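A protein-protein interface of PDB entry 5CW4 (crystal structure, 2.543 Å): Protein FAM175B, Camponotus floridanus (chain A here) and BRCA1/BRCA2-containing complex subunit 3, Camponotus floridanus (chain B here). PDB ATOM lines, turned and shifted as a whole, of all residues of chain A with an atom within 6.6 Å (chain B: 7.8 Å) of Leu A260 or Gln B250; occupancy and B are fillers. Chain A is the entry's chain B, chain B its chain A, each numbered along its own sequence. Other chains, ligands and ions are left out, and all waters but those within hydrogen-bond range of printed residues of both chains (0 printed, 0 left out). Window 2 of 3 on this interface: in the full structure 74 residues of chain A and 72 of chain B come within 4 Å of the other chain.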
ATOM      1  N   LYS A 255       5.674  -3.362  14.184  1.00  0.00           N
ATOM      2  CA  LYS A 255       4.805  -4.152  15.045  1.00  0.00           C
ATOM      3  C   LYS A 255       5.267  -5.607  15.126  1.00  0.00           C
ATOM      4  O   LYS A 255       5.316  -6.189  16.210  1.00  0.00           O
ATOM      5  CB  LYS A 255       3.364  -4.077  14.538  1.00  0.00           C
ATOM      6  CG  LYS A 255       2.325  -4.715  15.447  1.00  0.00           C
ATOM      7  CD  LYS A 255       0.920  -4.482  14.897  1.00  0.00           C
ATOM      8  CE  LYS A 255      -0.151  -5.080  15.795  1.00  0.00           C
ATOM      9  NZ  LYS A 255      -0.035  -6.561  15.896  1.00  0.00           N
ATOM     10  N   GLN A 256       5.609  -6.185  13.976  1.00  0.00           N
ATOM     11  CA  GLN A 256       6.044  -7.578  13.911  1.00  0.00           C
ATOM     12  C   GLN A 256       7.383  -7.792  14.609  1.00  0.00           C
ATOM     13  O   GLN A 256       7.588  -8.805  15.280  1.00  0.00           O
ATOM     14  CB  GLN A 256       6.145  -8.046  12.458  1.00  0.00           C
ATOM     15  CG  GLN A 256       4.818  -8.083  11.719  1.00  0.00           C
ATOM     16  CD  GLN A 256       4.958  -8.575  10.290  1.00  0.00           C
ATOM     17  OE1 GLN A 256       5.860  -9.351   9.972  1.00  0.00           O
ATOM     18  NE2 GLN A 256       4.066  -8.119   9.419  1.00  0.00           N
ATOM     19  N   VAL A 257       8.298  -6.843  14.443  1.00  0.00           N
ATOM     20  CA  VAL A 257       9.611  -6.952  15.060  1.00  0.00           C
ATOM     21  C   VAL A 257       9.527  -6.804  16.576  1.00  0.00           C
ATOM     22  O   VAL A 257      10.187  -7.540  17.311  1.00  0.00           O
ATOM     23  CB  VAL A 257      10.590  -5.908  14.494  1.00  0.00           C
ATOM     24  CG1 VAL A 257      11.693  -5.602  15.501  1.00  0.00           C
ATOM     25  CG2 VAL A 257      11.178  -6.397  13.180  1.00  0.00           C
ATOM     26  N   HIS A 258       8.712  -5.863  17.044  1.00  0.00           N
ATOM     27  CA  HIS A 258       8.583  -5.629  18.480  1.00  0.00           C
ATOM     28  C   HIS A 258       8.036  -6.851  19.208  1.00  0.00           C
ATOM     29  O   HIS A 258       8.432  -7.143  20.336  1.00  0.00           O
ATOM     30  CB  HIS A 258       7.683  -4.427  18.763  1.00  0.00           C
ATOM     31  CG  HIS A 258       7.503  -4.149  20.222  1.00  0.00           C
ATOM     32  ND1 HIS A 258       6.317  -4.377  20.884  1.00  0.00           N
ATOM     33  CD2 HIS A 258       8.368  -3.676  21.152  1.00  0.00           C
ATOM     34  CE1 HIS A 258       6.454  -4.047  22.158  1.00  0.00           C
ATOM     35  NE2 HIS A 258       7.690  -3.620  22.345  1.00  0.00           N
ATOM     36  N   GLU A 259       7.121  -7.562  18.558  1.00  0.00           N
ATOM     37  CA  GLU A 259       6.484  -8.722  19.167  1.00  0.00           C
ATOM     38  C   GLU A 259       7.457  -9.890  19.304  1.00  0.00           C
ATOM     39  O   GLU A 259       7.510 -10.538  20.350  1.00  0.00           O
ATOM     40  CB  GLU A 259       5.254  -9.136  18.359  1.00  0.00           C
ATOM     41  CG  GLU A 259       4.121  -8.120  18.427  1.00  0.00           C
ATOM     42  CD  GLU A 259       2.893  -8.549  17.648  1.00  0.00           C
ATOM     43  OE1 GLU A 259       2.993  -9.515  16.862  1.00  0.00           O
ATOM     44  OE2 GLU A 259       1.827  -7.920  17.822  1.00  0.00           O
ATOM     45  N   LEU A 260       8.230 -10.150  18.254  1.00  0.00           N
ATOM     46  CA  LEU A 260       9.245 -11.198  18.298  1.00  0.00           C
ATOM     47  C   LEU A 260      10.284 -10.919  19.379  1.00  0.00           C
ATOM     48  O   LEU A 260      10.631 -11.809  20.155  1.00  0.00           O
ATOM     49  CB  LEU A 260       9.928 -11.347  16.939  1.00  0.00           C
ATOM     50  CG  LEU A 260       9.147 -12.137  15.889  1.00  0.00           C
ATOM     51  CD1 LEU A 260       9.993 -12.355  14.643  1.00  0.00           C
ATOM     52  CD2 LEU A 260       8.672 -13.466  16.460  1.00  0.00           C
ATOM     53  N   LYS A 261      10.775  -9.682  19.420  1.00  0.00           N
ATOM     54  CA  LYS A 261      11.739  -9.266  20.436  1.00  0.00           C
ATOM     55  C   LYS A 261      11.224  -9.546  21.845  1.00  0.00           C
ATOM     56  O   LYS A 261      11.986  -9.954  22.720  1.00  0.00           O
ATOM     57  CB  LYS A 261      12.066  -7.780  20.295  1.00  0.00           C
ATOM     58  CG  LYS A 261      13.004  -7.437  19.154  1.00  0.00           C
ATOM     59  CD  LYS A 261      13.264  -5.941  19.120  1.00  0.00           C
ATOM     60  CE  LYS A 261      14.232  -5.559  18.015  1.00  0.00           C
ATOM     61  NZ  LYS A 261      14.468  -4.087  17.989  1.00  0.00           N
ATOM     62  N   ILE A 262       9.931  -9.318  22.058  1.00  0.00           N
ATOM     63  CA  ILE A 262       9.314  -9.616  23.345  1.00  0.00           C
ATOM     64  C   ILE A 262       9.180 -11.125  23.542  1.00  0.00           C
ATOM     65  O   ILE A 262       9.344 -11.634  24.650  1.00  0.00           O
ATOM     66  CB  ILE A 262       7.928  -8.963  23.477  1.00  0.00           C
ATOM     67  CG1 ILE A 262       8.050  -7.442  23.398  1.00  0.00           C
ATOM     68  CG2 ILE A 262       7.273  -9.370  24.789  1.00  0.00           C
ATOM     69  CD1 ILE A 262       8.823  -6.832  24.551  1.00  0.00           C
ATOM     70  N   LYS A 263       8.878 -11.832  22.458  1.00  0.00           N
ATOM     71  CA  LYS A 263       8.740 -13.283  22.500  1.00  0.00           C
ATOM     72  C   LYS A 263      10.072 -13.935  22.846  1.00  0.00           C
ATOM     73  O   LYS A 263      10.129 -14.886  23.625  1.00  0.00           O
ATOM     74  CB  LYS A 263       8.221 -13.810  21.162  1.00  0.00           C
ATOM     75  CG  LYS A 263       8.104 -15.321  21.088  1.00  0.00           C
ATOM     76  CD  LYS A 263       7.600 -15.759  19.723  1.00  0.00           C
ATOM     77  CE  LYS A 263       7.538 -17.270  19.610  1.00  0.00           C
ATOM     78  NZ  LYS A 263       7.033 -17.697  18.277  1.00  0.00           N
ATOM     79  N   ILE A 264      11.143 -13.412  22.262  1.00  0.00           N
ATOM     80  CA  ILE A 264      12.484 -13.908  22.534  1.00  0.00           C
ATOM     81  C   ILE A 264      12.949 -13.493  23.927  1.00  0.00           C
ATOM     82  O   ILE A 264      13.605 -14.261  24.626  1.00  0.00           O
ATOM     83  CB  ILE A 264      13.488 -13.396  21.486  1.00  0.00           C
ATOM     84  CG1 ILE A 264      13.150 -13.971  20.109  1.00  0.00           C
ATOM     85  CG2 ILE A 264      14.910 -13.754  21.887  1.00  0.00           C
ATOM     86  CD1 ILE A 264      13.984 -13.400  18.987  1.00  0.00           C
ATOM     87  N   ALA A 265      12.596 -12.274  24.321  1.00  0.00           N
ATOM     88  CA  ALA A 265      13.006 -11.726  25.610  1.00  0.00           C
ATOM     89  C   ALA A 265      12.454 -12.534  26.778  1.00  0.00           C
ATOM     90  O   ALA A 265      13.162 -12.784  27.753  1.00  0.00           O
ATOM     91  CB  ALA A 265      12.571 -10.273  25.727  1.00  0.00           C
ATOM     92  N   GLN B 243      13.015  -5.802   8.096  1.00  0.00           N
ATOM     93  CA  GLN B 243      12.832  -7.105   7.465  1.00  0.00           C
ATOM     94  C   GLN B 243      14.045  -8.012   7.648  1.00  0.00           C
ATOM     95  O   GLN B 243      13.894  -9.196   7.944  1.00  0.00           O
ATOM     96  CB  GLN B 243      12.518  -6.939   5.978  1.00  0.00           C
ATOM     97  CG  GLN B 243      11.032  -6.820   5.687  1.00  0.00           C
ATOM     98  CD  GLN B 243      10.742  -6.197   4.338  1.00  0.00           C
ATOM     99  OE1 GLN B 243      11.611  -5.570   3.731  1.00  0.00           O
ATOM    100  NE2 GLN B 243       9.511  -6.360   3.864  1.00  0.00           N
ATOM    101  N   ARG B 244      15.244  -7.460   7.473  1.00  0.00           N
ATOM    102  CA  ARG B 244      16.466  -8.222   7.718  1.00  0.00           C
ATOM    103  C   ARG B 244      16.509  -8.685   9.170  1.00  0.00           C
ATOM    104  O   ARG B 244      16.949  -9.793   9.473  1.00  0.00           O
ATOM    105  CB  ARG B 244      17.711  -7.392   7.395  1.00  0.00           C
ATOM    106  CG  ARG B 244      17.851  -7.006   5.932  1.00  0.00           C
ATOM    107  CD  ARG B 244      19.228  -6.429   5.644  1.00  0.00           C
ATOM    108  NE  ARG B 244      19.580  -5.349   6.563  1.00  0.00           N
ATOM    109  CZ  ARG B 244      19.284  -4.067   6.367  1.00  0.00           C
ATOM    110  NH1 ARG B 244      18.624  -3.694   5.278  1.00  0.00           N
ATOM    111  NH2 ARG B 244      19.647  -3.155   7.260  1.00  0.00           N
ATOM    112  N   GLN B 245      16.034  -7.822  10.059  1.00  0.00           N
ATOM    113  CA  GLN B 245      16.013  -8.102  11.485  1.00  0.00           C
ATOM    114  C   GLN B 245      14.945  -9.138  11.808  1.00  0.00           C
ATOM    115  O   GLN B 245      15.064  -9.894  12.775  1.00  0.00           O
ATOM    116  CB  GLN B 245      15.765  -6.809  12.264  1.00  0.00           C
ATOM    117  CG  GLN B 245      16.163  -6.847  13.725  1.00  0.00           C
ATOM    118  CD  GLN B 245      16.008  -5.491  14.388  1.00  0.00           C
ATOM    119  OE1 GLN B 245      15.486  -4.552  13.786  1.00  0.00           O
ATOM    120  NE2 GLN B 245      16.463  -5.379  15.629  1.00  0.00           N
ATOM    121  N   LEU B 246      13.904  -9.173  10.982  1.00  0.00           N
ATOM    122  CA  LEU B 246      12.767 -10.063  11.201  1.00  0.00           C
ATOM    123  C   LEU B 246      13.128 -11.523  10.936  1.00  0.00           C
ATOM    124  O   LEU B 246      12.563 -12.432  11.544  1.00  0.00           O
ATOM    125  CB  LEU B 246      11.592  -9.640  10.316  1.00  0.00           C
ATOM    126  CG  LEU B 246      10.217 -10.222  10.642  1.00  0.00           C
ATOM    127  CD1 LEU B 246       9.831  -9.907  12.076  1.00  0.00           C
ATOM    128  CD2 LEU B 246       9.177  -9.679   9.674  1.00  0.00           C
ATOM    129  N   GLN B 247      14.073 -11.743  10.026  1.00  0.00           N
ATOM    130  CA  GLN B 247      14.526 -13.092   9.708  1.00  0.00           C
ATOM    131  C   GLN B 247      15.397 -13.656  10.823  1.00  0.00           C
ATOM    132  O   GLN B 247      15.335 -14.845  11.137  1.00  0.00           O
ATOM    133  CB  GLN B 247      15.304 -13.101   8.392  1.00  0.00           C
ATOM    134  CG  GLN B 247      14.484 -12.735   7.168  1.00  0.00           C
ATOM    135  CD  GLN B 247      15.313 -12.748   5.897  1.00  0.00           C
ATOM    136  OE1 GLN B 247      16.468 -12.321   5.891  1.00  0.00           O
ATOM    137  NE2 GLN B 247      14.729 -13.247   4.813  1.00  0.00           N
ATOM    138  N   GLU B 248      16.212 -12.788  11.416  1.00  0.00           N
ATOM    139  CA  GLU B 248      17.146 -13.188  12.461  1.00  0.00           C
ATOM    140  C   GLU B 248      16.427 -13.549  13.758  1.00  0.00           C
ATOM    141  O   GLU B 248      16.849 -14.451  14.481  1.00  0.00           O
ATOM    142  CB  GLU B 248      18.156 -12.070  12.717  1.00  0.00           C
ATOM    143  CG  GLU B 248      18.916 -11.631  11.477  1.00  0.00           C
ATOM    144  CD  GLU B 248      19.493 -10.236  11.612  1.00  0.00           C
ATOM    145  OE1 GLU B 248      20.252  -9.814  10.714  1.00  0.00           O
ATOM    146  OE2 GLU B 248      19.181  -9.556  12.613  1.00  0.00           O
ATOM    147  N   LEU B 249      15.341 -12.842  14.046  1.00  0.00           N
ATOM    148  CA  LEU B 249      14.594 -13.066  15.279  1.00  0.00           C
ATOM    149  C   LEU B 249      13.768 -14.350  15.220  1.00  0.00           C
ATOM    150  O   LEU B 249      13.563 -15.009  16.238  1.00  0.00           O
ATOM    151  CB  LEU B 249      13.688 -11.870  15.575  1.00  0.00           C
ATOM    152  CG  LEU B 249      14.418 -10.532  15.706  1.00  0.00           C
ATOM    153  CD1 LEU B 249      13.473  -9.448  16.199  1.00  0.00           C
ATOM    154  CD2 LEU B 249      15.625 -10.660  16.626  1.00  0.00           C
ATOM    155  N   GLN B 250      13.294 -14.696  14.027  1.00  0.00           N
ATOM    156  CA  GLN B 250      12.540 -15.930  13.835  1.00  0.00           C
ATOM    157  C   GLN B 250      13.463 -17.134  13.971  1.00  0.00           C
ATOM    158  O   GLN B 250      13.033 -18.217  14.370  1.00  0.00           O
ATOM    159  CB  GLN B 250      11.844 -15.932  12.472  1.00  0.00           C
ATOM    160  CG  GLN B 250      10.675 -14.959  12.377  1.00  0.00           C
ATOM    161  CD  GLN B 250      10.234 -14.702  10.947  1.00  0.00           C
ATOM    162  OE1 GLN B 250      11.016 -14.844  10.008  1.00  0.00           O
ATOM    163  NE2 GLN B 250       8.973 -14.317  10.776  1.00  0.00           N
ATOM    164  N   LYS B 251      14.736 -16.935  13.640  1.00  0.00           N
ATOM    165  CA  LYS B 251      15.742 -17.978  13.809  1.00  0.00           C
ATOM    166  C   LYS B 251      15.976 -18.250  15.292  1.00  0.00           C
ATOM    167  O   LYS B 251      16.288 -19.373  15.688  1.00  0.00           O
ATOM    168  CB  LYS B 251      17.053 -17.582  13.124  1.00  0.00           C
ATOM    169  N   MET B 252      15.816 -17.211  16.105  1.00  0.00           N
ATOM    170  CA  MET B 252      15.977 -17.319  17.550  1.00  0.00           C
ATOM    171  C   MET B 252      14.885 -18.194  18.161  1.00  0.00           C
ATOM    172  O   MET B 252      15.100 -18.858  19.178  1.00  0.00           O
ATOM    173  CB  MET B 252      15.958 -15.932  18.194  1.00  0.00           C
ATOM    174  CG  MET B 252      16.987 -14.964  17.627  1.00  0.00           C
ATOM    175  SD  MET B 252      18.791 -15.333  18.258  1.00  0.00           S
ATOM    176  CE  MET B 252      18.519 -14.971  20.155  1.00  0.00           C
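The side-chain amide nitrogen of Gln B245 lies close to the side-chain amino group of Lys A261, at 3.3 Å.
O of Leu B246 sits close to OE1 of Gln B250 (3.3 Å).
Among the printed residues, merely in contact across the chains: Ile A264 with Leu B249, Ile A264 with Met B252, Gln A256 with Leu B246, Leu A260 with Gln B250, Leu A260 with Leu B246, Lys A261 with Leu B249, Leu A260 with Leu B249, Val A257 with Leu B246 and Val A257 with Leu B249.
Printed residues of chain B within 4 Å of Gln A256: Leu B246 (3.3 Å). Of chain B, only Leu B246 (3.6 Å), Leu B249 (3.8 Å) and Gln B250 (3.5 Å) come within 4 Å of Leu A260. Of the printed residues of chain B, Lys A261 touches Gln B245 (3.3 Å) and Leu B249 (3.6 Å). Printed residues of chain A within 4 Å of Leu B249: Val A257, Leu A260, Lys A261 and Ile A264. Gln B250 touches one residue of chain A. Printed residues of chain A within 4 Å of Met B252: Ile A264. The nearest residue of chain A that does not touch Gln B250 is Ile A264 (5.2 Å). The nearest printed residue of chain A that does not touch Met B252 is Leu A260 (7.0 Å).
Printed residues of chain A that touch a printed residue of chain B: Gln A256, Val A257, Leu A260, Lys A261 and Ile A264. Of the 10 printed residues of chain B, 5 touch a printed residue of chain A. Printed residues of chain B that touch a printed residue of chain A: Gln B245, Leu B246, Leu B249, Gln B250 and Met B252. Hydrophobic or aromatic side chains of chain B within 4 Å of the printed part of chain A: Leu B246, Leu B249 and Met B252. Among the printed residues, no Asp or Glu carboxylate lies within 4 Å of a Lys or Arg side-chain nitrogen of the other chain.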
